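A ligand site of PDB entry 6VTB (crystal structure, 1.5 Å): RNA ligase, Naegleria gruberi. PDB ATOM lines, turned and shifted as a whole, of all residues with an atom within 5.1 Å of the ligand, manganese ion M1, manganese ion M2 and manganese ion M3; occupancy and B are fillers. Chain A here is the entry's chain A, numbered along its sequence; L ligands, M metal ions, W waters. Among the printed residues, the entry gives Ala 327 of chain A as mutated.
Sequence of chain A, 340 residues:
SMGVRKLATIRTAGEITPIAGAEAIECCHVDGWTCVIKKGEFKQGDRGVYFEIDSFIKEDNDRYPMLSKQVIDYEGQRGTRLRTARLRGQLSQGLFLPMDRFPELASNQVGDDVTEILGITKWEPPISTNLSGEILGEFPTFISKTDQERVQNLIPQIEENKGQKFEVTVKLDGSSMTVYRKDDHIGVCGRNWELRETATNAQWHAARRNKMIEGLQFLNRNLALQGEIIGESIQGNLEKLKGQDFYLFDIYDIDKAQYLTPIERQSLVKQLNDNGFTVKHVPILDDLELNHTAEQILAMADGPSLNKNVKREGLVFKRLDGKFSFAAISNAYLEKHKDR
OE1 of Glu 228 sits at hydrogen-bond distance from O13 of the ligand, 2.6 Å away. O of Thr 146 lies within hydrogen-bond range of O12 of the ligand, 3.0 Å away. The side-chain hydroxyl of Thr 146 lies within hydrogen-bond range of an oxygen (O12) of the ligand (2.6 Å). The backbone NH (N) of Gln 148 is in hydrogen-bond range of an oxygen (O7) of the ligand. An oxygen (O11) of the ligand lies within hydrogen-bond range of the side-chain amino group of Lys 171, 3.1 Å away. The side-chain amino group of Lys 318 lies within hydrogen-bond range of a nitrogen (N4) of the ligand, at 2.9 Å. The side-chain hydroxyl (OG1) of Thr 169 lies within hydrogen-bond range of a nitrogen (N3) of the ligand (2.9 Å). The guanidinium group (NE) of Arg 191 is in salt-bridge range of an oxygen (O1) of the ligand, 3.1 Å away. The backbone carbonyl oxygen of Val 170 lies within hydrogen-bond range of a nitrogen (N3) of the ligand (3.0 Å). The backbone NH (N) of Leu 172 is in hydrogen-bond range of a nitrogen (N2) of the ligand, at 3.0 Å.
The guanidinium group of Arg 191 lies within salt-bridge range of the side-chain carboxylate of Glu 124 (3.4 Å). The side-chain carboxylate of Glu 228 sits at hydrogen-bond distance from the backbone NH of Gly 174, at 2.8 Å. The side-chain hydroxyl of Thr 146 sits at hydrogen-bond distance from the side-chain hydroxyl of Ser 176 (2.7 Å). The side-chain amino group (NZ) of Lys 171 lies within salt-bridge range of the side-chain carboxylate (OE2) of Glu 313 (2.8 Å). The side-chain hydroxyl (OG1) of Thr 169 lies within hydrogen-bond range of the side-chain amino group (NZ) of Lys 318 (3.2 Å). The backbone NH of Val 316 is in hydrogen-bond range of the backbone carbonyl oxygen of Thr 169 (2.8 Å). The backbone carbonyl oxygen of Ser 176 lies within hydrogen-bond range of the backbone NH of Arg 191 (3.3 Å). The side-chain carboxylate (OD2) of Asp 54 is in salt-bridge range of the guanidinium group (NH2) of Arg 150 (2.4 Å).
CA of Asp 147 touches O7 of the ligand, 3.4 Å away. CB of Ser 176 touches O13 of the ligand, at 3.2 Å. CB of Phe 249 touches N4 of the ligand, at 3.5 Å. Val 282 touches the ligand (CG2 to N3, 3.5 Å). Val 316 touches the ligand. Hydrophobic or aromatic side chains within 4 Å of the ligand: Phe 249, Val 282 and Val 316. 15 residues have an atom within 4 Å of the ligand: Glu 124, Thr 146, Asp 147, Gln 148, Thr 169, Val 170, Lys 171, Leu 172, Ser 176, Arg 191, Glu 228, Phe 249, Val 282, Val 316 and Lys 318.
Lys 171 touches manganese ion M1 (NZ to MN, 3.9 Å). Glu 228 touches manganese ion M1 (OE2 to MN, 3.999 Å). The nearest printed residue that does not touch manganese ion M1 is Glu 313 (4.2 Å).
Within 4 Å of manganese ion M2: Glu 124.
Arg 150 touches manganese ion M3. The nearest printed residue that does not touch manganese ion M3 is Asp 54 (4.4 Å).
Manganese ion M1 is bound by an oxygen (O5) of the ligand, an oxygen (O3) of the ligand, water W5, water W14, water W3 and water W1. Manganese ion M1 has six donor atoms within binding distance.
Manganese ion M2 is bound by water W4 (2.1 Å), an oxygen (O2) of the ligand (2.1 Å), water W19 (2.1 Å), water W10 (2.1 Å), the side-chain carboxylate of Glu 124 (2.2 Å) and water W6 (2.2 Å). Slightly farther from manganese ion M2 lies the side-chain carboxylate (OE2) of Glu 124 (2.8 Å).
Manganese ion M3 is bound by O4 of the ligand (1.9 Å), water W7 (2.1 Å), O8 of the ligand (2.2 Å), water W9 (2.3 Å), water W15 (2.4 Å) and water W8 (2.4 Å). Manganese ion M3 has six donor atoms within binding distance.
Water W14 bridges OE2 of Glu 228 and O13 of the ligand. Water W5 lies within hydrogen-bond range of the side-chain carboxylate of Asp 173 (2.7 Å), the backbone carbonyl oxygen of Gly 174 (2.7 Å) and the side-chain amide nitrogen of Gln 235 (3.3 Å). Water W15 lies within hydrogen-bond range of the side-chain carboxylate of Glu 313 (3.1 Å) and the side-chain amino group of Lys 171 (3.3 Å). Water W13 lies within hydrogen-bond range of O7 of the ligand (2.6 Å), O of Ser 1 (2.8 Å), N of Gly 3 (2.9 Å) and O of Gln 148 (3.2 Å). Water W20 lies within hydrogen-bond range of O of Gly 174 and O1 of the ligand. Water W11 lies within hydrogen-bond range of O of Thr 146 (2.7 Å), NE2 of Gln 148 (3.0 Å) and N5 of the ligand (3.2 Å).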
ATOM      1  N   SER A   1      36.622   2.615  31.021  1.00  0.00           N
ATOM      2  CA  SER A   1      36.967   1.332  31.628  1.00  0.00           C
ATOM      3  C   SER A   1      36.786   0.209  30.608  1.00  0.00           C
ATOM      4  O   SER A   1      36.423   0.460  29.455  1.00  0.00           O
ATOM      5  CB  SER A   1      36.087   1.084  32.859  1.00  0.00           C
ATOM      6  OG  SER A   1      34.730   1.070  32.502  1.00  0.00           O
ATOM      7  N   GLY A   3      34.537  -2.853  30.744  1.00  0.00           N
ATOM      8  CA  GLY A   3      33.580  -3.585  31.546  1.00  0.00           C
ATOM      9  C   GLY A   3      33.838  -3.317  33.014  1.00  0.00           C
ATOM     10  O   GLY A   3      33.989  -2.164  33.436  1.00  0.00           O
ATOM     11  N   ASP A  54      30.973   5.883  36.948  1.00  0.00           N
ATOM     12  CA  ASP A  54      30.261   4.610  37.007  1.00  0.00           C
ATOM     13  C   ASP A  54      30.848   3.691  38.071  1.00  0.00           C
ATOM     14  O   ASP A  54      30.248   2.650  38.342  1.00  0.00           O
ATOM     15  CB  ASP A  54      30.213   3.847  35.669  1.00  0.00           C
ATOM     16  CG  ASP A  54      29.728   4.708  34.503  1.00  0.00           C
ATOM     17  OD1 ASP A  54      28.859   5.590  34.728  1.00  0.00           O
ATOM     18  OD2 ASP A  54      30.228   4.505  33.378  1.00  0.00           O
ATOM     19  N   LYS A 122      30.956  -1.789  39.375  1.00  0.00           N
ATOM     20  CA  LYS A 122      30.391  -0.857  38.402  1.00  0.00           C
ATOM     21  C   LYS A 122      28.903  -0.709  38.670  1.00  0.00           C
ATOM     22  O   LYS A 122      28.168  -1.704  38.697  1.00  0.00           O
ATOM     23  CB  LYS A 122      30.645  -1.325  36.970  1.00  0.00           C
ATOM     24  CG  LYS A 122      30.322  -0.284  35.922  1.00  0.00           C
ATOM     25  CD  LYS A 122      31.110  -0.525  34.640  1.00  0.00           C
ATOM     26  CE  LYS A 122      31.164   0.757  33.812  1.00  0.00           C
ATOM     27  NZ  LYS A 122      32.543   1.166  33.459  1.00  0.00           N
ATOM     28  N   TRP A 123      28.458   0.528  38.868  1.00  0.00           N
ATOM     29  CA  TRP A 123      27.039   0.793  39.019  1.00  0.00           C
ATOM     30  C   TRP A 123      26.301   0.514  37.711  1.00  0.00           C
ATOM     31  O   TRP A 123      26.782   0.856  36.621  1.00  0.00           O
ATOM     32  CB  TRP A 123      26.837   2.250  39.454  1.00  0.00           C
ATOM     33  CG  TRP A 123      25.408   2.628  39.692  1.00  0.00           C
ATOM     34  CD1 TRP A 123      24.749   2.623  40.889  1.00  0.00           C
ATOM     35  CD2 TRP A 123      24.471   3.087  38.717  1.00  0.00           C
ATOM     36  NE1 TRP A 123      23.447   3.037  40.713  1.00  0.00           N
ATOM     37  CE2 TRP A 123      23.253   3.314  39.384  1.00  0.00           C
ATOM     38  CE3 TRP A 123      24.543   3.305  37.335  1.00  0.00           C
ATOM     39  CZ2 TRP A 123      22.114   3.780  38.717  1.00  0.00           C
ATOM     40  CZ3 TRP A 123      23.408   3.748  36.677  1.00  0.00           C
ATOM     41  CH2 TRP A 123      22.208   3.983  37.368  1.00  0.00           C
ATOM     42  N   GLU A 124      25.126  -0.115  37.810  1.00  0.00           N
ATOM     43  CA  GLU A 124      24.302  -0.352  36.644  1.00  0.00           C
ATOM     44  C   GLU A 124      22.857   0.022  36.925  1.00  0.00           C
ATOM     45  O   GLU A 124      22.370  -0.149  38.043  1.00  0.00           O
ATOM     46  CB  GLU A 124      24.363  -1.833  36.232  1.00  0.00           C
ATOM     47  CG  GLU A 124      25.757  -2.330  35.854  1.00  0.00           C
ATOM     48  CD  GLU A 124      26.280  -1.676  34.603  1.00  0.00           C
ATOM     49  OE1 GLU A 124      25.478  -1.135  33.824  1.00  0.00           O
ATOM     50  OE2 GLU A 124      27.508  -1.720  34.384  1.00  0.00           O
ATOM     51  N   PRO A 125      22.137   0.520  35.922  1.00  0.00           N
ATOM     52  CA  PRO A 125      20.726   0.851  36.112  1.00  0.00           C
ATOM     53  C   PRO A 125      19.888  -0.411  36.196  1.00  0.00           C
ATOM     54  O   PRO A 125      20.383  -1.519  35.944  1.00  0.00           O
ATOM     55  CB  PRO A 125      20.390   1.670  34.854  1.00  0.00           C
ATOM     56  CG  PRO A 125      21.323   1.170  33.835  1.00  0.00           C
ATOM     57  CD  PRO A 125      22.596   0.821  34.560  1.00  0.00           C
ATOM     58  N   THR A 146      32.017  -7.211  24.425  1.00  0.00           N
ATOM     59  CA  THR A 146      31.807  -6.023  23.596  1.00  0.00           C
ATOM     60  C   THR A 146      32.229  -4.725  24.281  1.00  0.00           C
ATOM     61  O   THR A 146      31.882  -3.650  23.788  1.00  0.00           O
ATOM     62  CB  THR A 146      30.342  -5.943  23.154  1.00  0.00           C
ATOM     63  OG1 THR A 146      29.490  -5.901  24.305  1.00  0.00           O
ATOM     64  CG2 THR A 146      29.988  -7.180  22.324  1.00  0.00           C
ATOM     65  N   ASP A 147      32.979  -4.799  25.376  1.00  0.00           N
ATOM     66  CA  ASP A 147      33.448  -3.598  26.065  1.00  0.00           C
ATOM     67  C   ASP A 147      34.241  -2.699  25.138  1.00  0.00           C
ATOM     68  O   ASP A 147      35.010  -3.171  24.294  1.00  0.00           O
ATOM     69  CB  ASP A 147      34.330  -3.977  27.265  1.00  0.00           C
ATOM     70  CG  ASP A 147      33.705  -5.030  28.145  1.00  0.00           C
ATOM     71  OD1 ASP A 147      32.564  -4.821  28.610  1.00  0.00           O
ATOM     72  OD2 ASP A 147      34.367  -6.070  28.376  1.00  0.00           O
ATOM     73  N   GLN A 148      34.079  -1.389  25.317  1.00  0.00           N
ATOM     74  CA  GLN A 148      34.833  -0.373  24.602  1.00  0.00           C
ATOM     75  C   GLN A 148      35.449   0.588  25.609  1.00  0.00           C
ATOM     76  O   GLN A 148      34.774   1.036  26.542  1.00  0.00           O
ATOM     77  CB  GLN A 148      33.958   0.413  23.629  1.00  0.00           C
ATOM     78  CG  GLN A 148      33.401  -0.401  22.462  1.00  0.00           C
ATOM     79  CD  GLN A 148      34.439  -0.728  21.421  1.00  0.00           C
ATOM     80  OE1 GLN A 148      35.524  -0.135  21.392  1.00  0.00           O
ATOM     81  NE2 GLN A 148      34.144  -1.704  20.562  1.00  0.00           N
ATOM     82  N   ARG A 150      36.971   4.215  26.771  1.00  0.00           N
ATOM     83  CA  ARG A 150      36.637   5.616  26.536  1.00  0.00           C
ATOM     84  C   ARG A 150      37.825   6.398  25.972  1.00  0.00           C
ATOM     85  O   ARG A 150      38.972   6.181  26.366  1.00  0.00           O
ATOM     86  CB  ARG A 150      36.219   6.293  27.846  1.00  0.00           C
ATOM     87  CG  ARG A 150      34.921   5.774  28.448  1.00  0.00           C
ATOM     88  CD  ARG A 150      34.572   6.516  29.724  1.00  0.00           C
ATOM     89  NE  ARG A 150      33.637   5.775  30.575  1.00  0.00           N
ATOM     90  CZ  ARG A 150      32.373   6.119  30.789  1.00  0.00           C
ATOM     91  NH1 ARG A 150      31.862   7.201  30.219  1.00  0.00           N
ATOM     92  NH2 ARG A 150      31.614   5.376  31.581  1.00  0.00           N
ATOM     93  N   THR A 169      30.287   4.773  14.181  1.00  0.00           N
ATOM     94  CA  THR A 169      28.904   4.353  14.327  1.00  0.00           C
ATOM     95  C   THR A 169      28.262   5.022  15.534  1.00  0.00           C
ATOM     96  O   THR A 169      28.928   5.380  16.513  1.00  0.00           O
ATOM     97  CB  THR A 169      28.764   2.817  14.471  1.00  0.00           C
ATOM     98  OG1 THR A 169      29.675   2.337  15.470  1.00  0.00           O
ATOM     99  CG2 THR A 169      29.043   2.118  13.141  1.00  0.00           C
ATOM    100  N   VAL A 170      26.937   5.156  15.448  1.00  0.00           N
ATOM    101  CA  VAL A 170      26.173   5.650  16.582  1.00  0.00           C
ATOM    102  C   VAL A 170      26.153   4.582  17.668  1.00  0.00           C
ATOM    103  O   VAL A 170      25.869   3.402  17.414  1.00  0.00           O
ATOM    104  CB  VAL A 170      24.746   6.020  16.147  1.00  0.00           C
ATOM    105  CG1 VAL A 170      23.898   6.332  17.352  1.00  0.00           C
ATOM    106  CG2 VAL A 170      24.786   7.217  15.188  1.00  0.00           C
ATOM    107  N   LYS A 171      26.434   5.009  18.899  1.00  0.00           N
ATOM    108  CA  LYS A 171      26.352   4.138  20.072  1.00  0.00           C
ATOM    109  C   LYS A 171      24.899   4.129  20.533  1.00  0.00           C
ATOM    110  O   LYS A 171      24.376   5.148  20.989  1.00  0.00           O
ATOM    111  CB  LYS A 171      27.273   4.643  21.174  1.00  0.00           C
ATOM    112  CG  LYS A 171      27.521   3.606  22.268  1.00  0.00           C
ATOM    113  CD  LYS A 171      28.596   4.095  23.220  1.00  0.00           C
ATOM    114  CE  LYS A 171      29.071   2.996  24.158  1.00  0.00           C
ATOM    115  NZ  LYS A 171      28.039   2.617  25.167  1.00  0.00           N
ATOM    116  N   LEU A 172      24.244   2.982  20.390  1.00  0.00           N
ATOM    117  CA  LEU A 172      22.866   2.822  20.799  1.00  0.00           C
ATOM    118  C   LEU A 172      22.794   2.435  22.269  1.00  0.00           C
ATOM    119  O   LEU A 172      23.650   1.711  22.776  1.00  0.00           O
ATOM    120  CB  LEU A 172      22.163   1.750  19.953  1.00  0.00           C
ATOM    121  CG  LEU A 172      22.047   2.072  18.467  1.00  0.00           C
ATOM    122  CD1 LEU A 172      21.290   0.951  17.769  1.00  0.00           C
ATOM    123  CD2 LEU A 172      21.329   3.398  18.265  1.00  0.00           C
ATOM    124  N   ASP A 173      21.747   2.892  22.950  1.00  0.00           N
ATOM    125  CA  ASP A 173      21.617   2.697  24.403  1.00  0.00           C
ATOM    126  C   ASP A 173      20.624   1.574  24.647  1.00  0.00           C
ATOM    127  O   ASP A 173      19.417   1.787  24.799  1.00  0.00           O
ATOM    128  CB  ASP A 173      21.183   3.997  25.069  1.00  0.00           C
ATOM    129  CG  ASP A 173      21.277   3.934  26.592  1.00  0.00           C
ATOM    130  OD1 ASP A 173      21.489   2.838  27.145  1.00  0.00           O
ATOM    131  OD2 ASP A 173      21.160   5.013  27.216  1.00  0.00           O
ATOM    132  N   GLY A 174      21.136   0.345  24.677  1.00  0.00           N
ATOM    133  CA  GLY A 174      20.324  -0.823  24.909  1.00  0.00           C
ATOM    134  C   GLY A 174      21.075  -1.832  25.753  1.00  0.00           C
ATOM    135  O   GLY A 174      21.670  -1.488  26.772  1.00  0.00           O
ATOM    136  N   SER A 175      21.087  -3.086  25.319  1.00  0.00           N
ATOM    137  CA  SER A 175      21.803  -4.141  26.027  1.00  0.00           C
ATOM    138  C   SER A 175      22.606  -4.940  25.005  1.00  0.00           C
ATOM    139  O   SER A 175      22.129  -5.243  23.916  1.00  0.00           O
ATOM    140  CB  SER A 175      20.824  -5.046  26.785  1.00  0.00           C
ATOM    141  OG  SER A 175      21.526  -5.856  27.716  1.00  0.00           O
ATOM    142  N   SER A 176      23.835  -5.283  25.382  1.00  0.00           N
ATOM    143  CA  SER A 176      24.705  -6.049  24.493  1.00  0.00           C
ATOM    144  C   SER A 176      24.220  -7.490  24.363  1.00  0.00           C
ATOM    145  O   SER A 176      23.950  -8.164  25.353  1.00  0.00           O
ATOM    146  CB  SER A 176      26.137  -6.047  24.999  1.00  0.00           C
ATOM    147  OG  SER A 176      26.958  -6.838  24.170  1.00  0.00           O
ATOM    148  N   ARG A 191      24.955  -9.705  28.081  1.00  0.00           N
ATOM    149  CA  ARG A 191      26.229  -9.030  28.293  1.00  0.00           C
ATOM    150  C   ARG A 191      27.246  -9.946  28.940  1.00  0.00           C
ATOM    151  O   ARG A 191      28.441  -9.870  28.635  1.00  0.00           O
ATOM    152  CB  ARG A 191      26.070  -7.789  29.161  1.00  0.00           C
ATOM    153  CG  ARG A 191      24.856  -6.947  28.897  1.00  0.00           C
ATOM    154  CD  ARG A 191      24.595  -6.042  30.096  1.00  0.00           C
ATOM    155  NE  ARG A 191      25.818  -5.428  30.591  1.00  0.00           N
ATOM    156  CZ  ARG A 191      25.859  -4.511  31.567  1.00  0.00           C
ATOM    157  NH1 ARG A 191      24.733  -4.105  32.140  1.00  0.00           N
ATOM    158  NH2 ARG A 191      27.021  -4.006  31.947  1.00  0.00           N
ATOM    159  N   GLU A 228      23.373  -4.562  19.650  1.00  0.00           N
ATOM    160  CA  GLU A 228      22.636  -3.935  20.737  1.00  0.00           C
ATOM    161  C   GLU A 228      21.162  -4.246  20.546  1.00  0.00           C
ATOM    162  O   GLU A 228      20.606  -3.980  19.470  1.00  0.00           O
ATOM    163  CB  GLU A 228      22.833  -2.427  20.747  1.00  0.00           C
ATOM    164  CG  GLU A 228      22.424  -1.756  22.048  1.00  0.00           C
ATOM    165  CD  GLU A 228      23.493  -1.877  23.123  1.00  0.00           C
ATOM    166  OE1 GLU A 228      24.386  -2.753  22.972  1.00  0.00           O
ATOM    167  OE2 GLU A 228      23.468  -1.097  24.087  1.00  0.00           O
ATOM    168  N   GLN A 235      16.363   0.427  28.899  1.00  0.00           N
ATOM    169  CA  GLN A 235      17.212   1.611  29.050  1.00  0.00           C
ATOM    170  C   GLN A 235      16.490   2.918  28.712  1.00  0.00           C
ATOM    171  O   GLN A 235      17.097   3.862  28.205  1.00  0.00           O
ATOM    172  CB  GLN A 235      18.483   1.497  28.186  1.00  0.00           C
ATOM    173  CG  GLN A 235      19.526   0.537  28.735  1.00  0.00           C
ATOM    174  CD  GLN A 235      20.187   1.089  29.981  1.00  0.00           C
ATOM    175  OE1 GLN A 235      19.640   0.975  31.077  1.00  0.00           O
ATOM    176  NE2 GLN A 235      21.356   1.723  29.818  1.00  0.00           N
ATOM    177  N   PHE A 249      26.753  -4.500  15.535  1.00  0.00           N
ATOM    178  CA  PHE A 249      27.899  -3.597  15.410  1.00  0.00           C
ATOM    179  C   PHE A 249      29.217  -4.316  15.232  1.00  0.00           C
ATOM    180  O   PHE A 249      30.212  -3.641  14.933  1.00  0.00           O
ATOM    181  CB  PHE A 249      27.998  -2.621  16.613  1.00  0.00           C
ATOM    182  CG  PHE A 249      27.935  -3.294  17.974  1.00  0.00           C
ATOM    183  CD1 PHE A 249      28.982  -4.103  18.430  1.00  0.00           C
ATOM    184  CD2 PHE A 249      26.831  -3.103  18.791  1.00  0.00           C
ATOM    185  CE1 PHE A 249      28.908  -4.726  19.666  1.00  0.00           C
ATOM    186  CE2 PHE A 249      26.748  -3.723  20.050  1.00  0.00           C
ATOM    187  CZ  PHE A 249      27.797  -4.534  20.476  1.00  0.00           C
ATOM    188  N   VAL A 282      23.787  -1.064  13.357  1.00  0.00           N
ATOM    189  CA  VAL A 282      23.803   0.260  13.991  1.00  0.00           C
ATOM    190  C   VAL A 282      24.024   1.323  12.918  1.00  0.00           C
ATOM    191  O   VAL A 282      24.618   1.023  11.877  1.00  0.00           O
ATOM    192  CB  VAL A 282      24.876   0.376  15.090  1.00  0.00           C
ATOM    193  CG1 VAL A 282      24.567  -0.557  16.284  1.00  0.00           C
ATOM    194  CG2 VAL A 282      26.290   0.117  14.539  1.00  0.00           C
ATOM    195  N   GLU A 313      23.601   8.654  22.630  1.00  0.00           N
ATOM    196  CA  GLU A 313      24.539   8.389  23.713  1.00  0.00           C
ATOM    197  C   GLU A 313      25.959   8.781  23.334  1.00  0.00           C
ATOM    198  O   GLU A 313      26.720   9.278  24.173  1.00  0.00           O
ATOM    199  CB  GLU A 313      24.479   6.905  24.089  1.00  0.00           C
ATOM    200  CG  GLU A 313      25.387   6.551  25.251  1.00  0.00           C
ATOM    201  CD  GLU A 313      25.525   5.053  25.463  1.00  0.00           C
ATOM    202  OE1 GLU A 313      24.740   4.276  24.881  1.00  0.00           O
ATOM    203  OE2 GLU A 313      26.413   4.671  26.224  1.00  0.00           O
ATOM    204  N   VAL A 316      30.932   5.094  18.484  1.00  0.00           N
ATOM    205  CA  VAL A 316      32.013   4.117  18.591  1.00  0.00           C
ATOM    206  C   VAL A 316      32.843   4.187  17.315  1.00  0.00           C
ATOM    207  O   VAL A 316      32.301   4.304  16.216  1.00  0.00           O
ATOM    208  CB  VAL A 316      31.510   2.677  18.855  1.00  0.00           C
ATOM    209  CG1 VAL A 316      32.687   1.725  18.983  1.00  0.00           C
ATOM    210  CG2 VAL A 316      30.644   2.653  20.128  1.00  0.00           C
ATOM    211  N   LYS A 318      35.825   2.323  15.092  1.00  0.00           N
ATOM    212  CA  LYS A 318      36.474   1.038  14.874  1.00  0.00           C
ATOM    213  C   LYS A 318      37.450   1.182  13.711  1.00  0.00           C
ATOM    214  O   LYS A 318      37.046   1.491  12.587  1.00  0.00           O
ATOM    215  CB  LYS A 318      35.436  -0.066  14.590  1.00  0.00           C
ATOM    216  CG  LYS A 318      34.428  -0.269  15.752  1.00  0.00           C
ATOM    217  CD  LYS A 318      33.409  -1.395  15.448  1.00  0.00           C
ATOM    218  CE  LYS A 318      32.298  -1.415  16.511  1.00  0.00           C
ATOM    219  NZ  LYS A 318      31.400  -0.214  16.366  1.00  0.00           N
ATOM    220  N   ALA A 327      35.177   4.279  22.365  1.00  0.00           N
ATOM    221  CA  ALA A 327      33.904   4.971  22.441  1.00  0.00           C
ATOM    222  C   ALA A 327      34.137   6.422  22.830  1.00  0.00           C
ATOM    223  O   ALA A 327      35.065   6.747  23.566  1.00  0.00           O
ATOM    224  CB  ALA A 327      32.975   4.305  23.457  1.00  0.00           C
HETATM  225  P1  LIG L   1      26.386  -1.309  29.597  1.00  0.00           P
HETATM  226  O1  LIG L   1      26.119  -2.706  29.091  1.00  0.00           O
HETATM  227  O2  LIG L   1      26.617  -1.212  31.095  1.00  0.00           O
HETATM  228  O3  LIG L   1      25.389  -0.288  29.049  1.00  0.00           O
HETATM  229  P2  LIG L   1      28.354   0.237  28.334  1.00  0.00           P
HETATM  230  O4  LIG L   1      28.673   1.223  29.422  1.00  0.00           O
HETATM  231  O5  LIG L   1      27.448   0.685  27.218  1.00  0.00           O
HETATM  232  O6  LIG L   1      27.855  -1.061  29.036  1.00  0.00           O
HETATM  233  P3  LIG L   1      30.950   0.329  27.088  1.00  0.00           P
HETATM  234  O7  LIG L   1      32.063  -0.655  27.164  1.00  0.00           O
HETATM  235  O8  LIG L   1      31.140   1.691  27.710  1.00  0.00           O
HETATM  236  O9  LIG L   1      29.686  -0.410  27.715  1.00  0.00           O
HETATM  237  O10 LIG L   1      30.501   0.591  25.573  1.00  0.00           O
HETATM  238  C1  LIG L   1      30.393  -0.535  24.705  1.00  0.00           C
HETATM  239  C2  LIG L   1      28.949  -0.995  24.629  1.00  0.00           C
HETATM  240  O11 LIG L   1      28.145  -0.164  23.784  1.00  0.00           O
HETATM  241  C3  LIG L   1      28.870  -2.364  23.998  1.00  0.00           C
HETATM  242  O12 LIG L   1      29.113  -3.386  24.986  1.00  0.00           O
HETATM  243  C4  LIG L   1      27.481  -2.416  23.391  1.00  0.00           C
HETATM  244  O13 LIG L   1      26.562  -2.928  24.351  1.00  0.00           O
HETATM  245  C5  LIG L   1      27.093  -0.969  23.182  1.00  0.00           C
HETATM  246  N1  LIG L   1      27.046  -0.430  21.809  1.00  0.00           N
HETATM  247  C6  LIG L   1      26.026   0.311  21.350  1.00  0.00           C
HETATM  248  N2  LIG L   1      26.256   0.757  20.106  1.00  0.00           N
HETATM  249  C7  LIG L   1      27.484   0.295  19.752  1.00  0.00           C
HETATM  250  C8  LIG L   1      28.319   0.429  18.558  1.00  0.00           C
HETATM  251  N3  LIG L   1      27.888   1.169  17.499  1.00  0.00           N
HETATM  252  N4  LIG L   1      29.517  -0.192  18.558  1.00  0.00           N
HETATM  253  C9  LIG L   1      29.943  -0.902  19.624  1.00  0.00           C
HETATM  254  N5  LIG L   1      29.221  -1.052  20.763  1.00  0.00           N
HETATM  255  C10 LIG L   1      28.006  -0.484  20.873  1.00  0.00           C
HETATM  256 MN    MN M   1      25.315   0.706  27.142  1.00  0.00          MN
HETATM  257 MN    MN M   2      26.700   0.233  32.591  1.00  0.00          MN
HETATM  258 MN    MN M   3      30.130   2.480  29.517  1.00  0.00          MN
HETATM  259  O   HOH W   1      25.286   1.648  25.105  1.00  0.00           O
HETATM  260  O   HOH W   2      33.498   3.126  27.526  1.00  0.00           O
HETATM  261  O   HOH W   3      25.345   2.779  27.987  1.00  0.00           O
HETATM  262  O   HOH W   4      25.096   1.065  31.602  1.00  0.00           O
HETATM  263  O   HOH W   5      23.159   0.745  27.187  1.00  0.00           O
HETATM  264  O   HOH W   6      26.893   1.715  34.235  1.00  0.00           O
HETATM  265  O   HOH W   7      31.774   1.599  30.478  1.00  0.00           O
HETATM  266  O   HOH W   8      29.388   3.136  31.728  1.00  0.00           O
HETATM  267  O   HOH W   9      31.211   4.385  28.705  1.00  0.00           O
HETATM  268  O   HOH W  10      28.668  -0.551  32.518  1.00  0.00           O
HETATM  269  O   HOH W  11      31.627  -3.154  21.135  1.00  0.00           O
HETATM  270  O   HOH W  12      30.164  -2.070  31.115  1.00  0.00           O
HETATM  271  O   HOH W  13      33.768  -0.510  29.144  1.00  0.00           O
HETATM  272  O   HOH W  14      25.105  -1.203  26.090  1.00  0.00           O
HETATM  273  O   HOH W  15      28.421   3.588  28.271  1.00  0.00           O
HETATM  274  O   HOH W  16      30.892  -2.961  28.780  1.00  0.00           O
HETATM  275  O   HOH W  17      28.086  -3.756  27.412  1.00  0.00           O
HETATM  276  O   HOH W  18      23.187  -0.225  30.785  1.00  0.00           O
HETATM  277  O   HOH W  19      27.219   1.862  31.346  1.00  0.00           O
HETATM  278  O   HOH W  20      23.111  -2.354  29.131  1.00  0.00           O
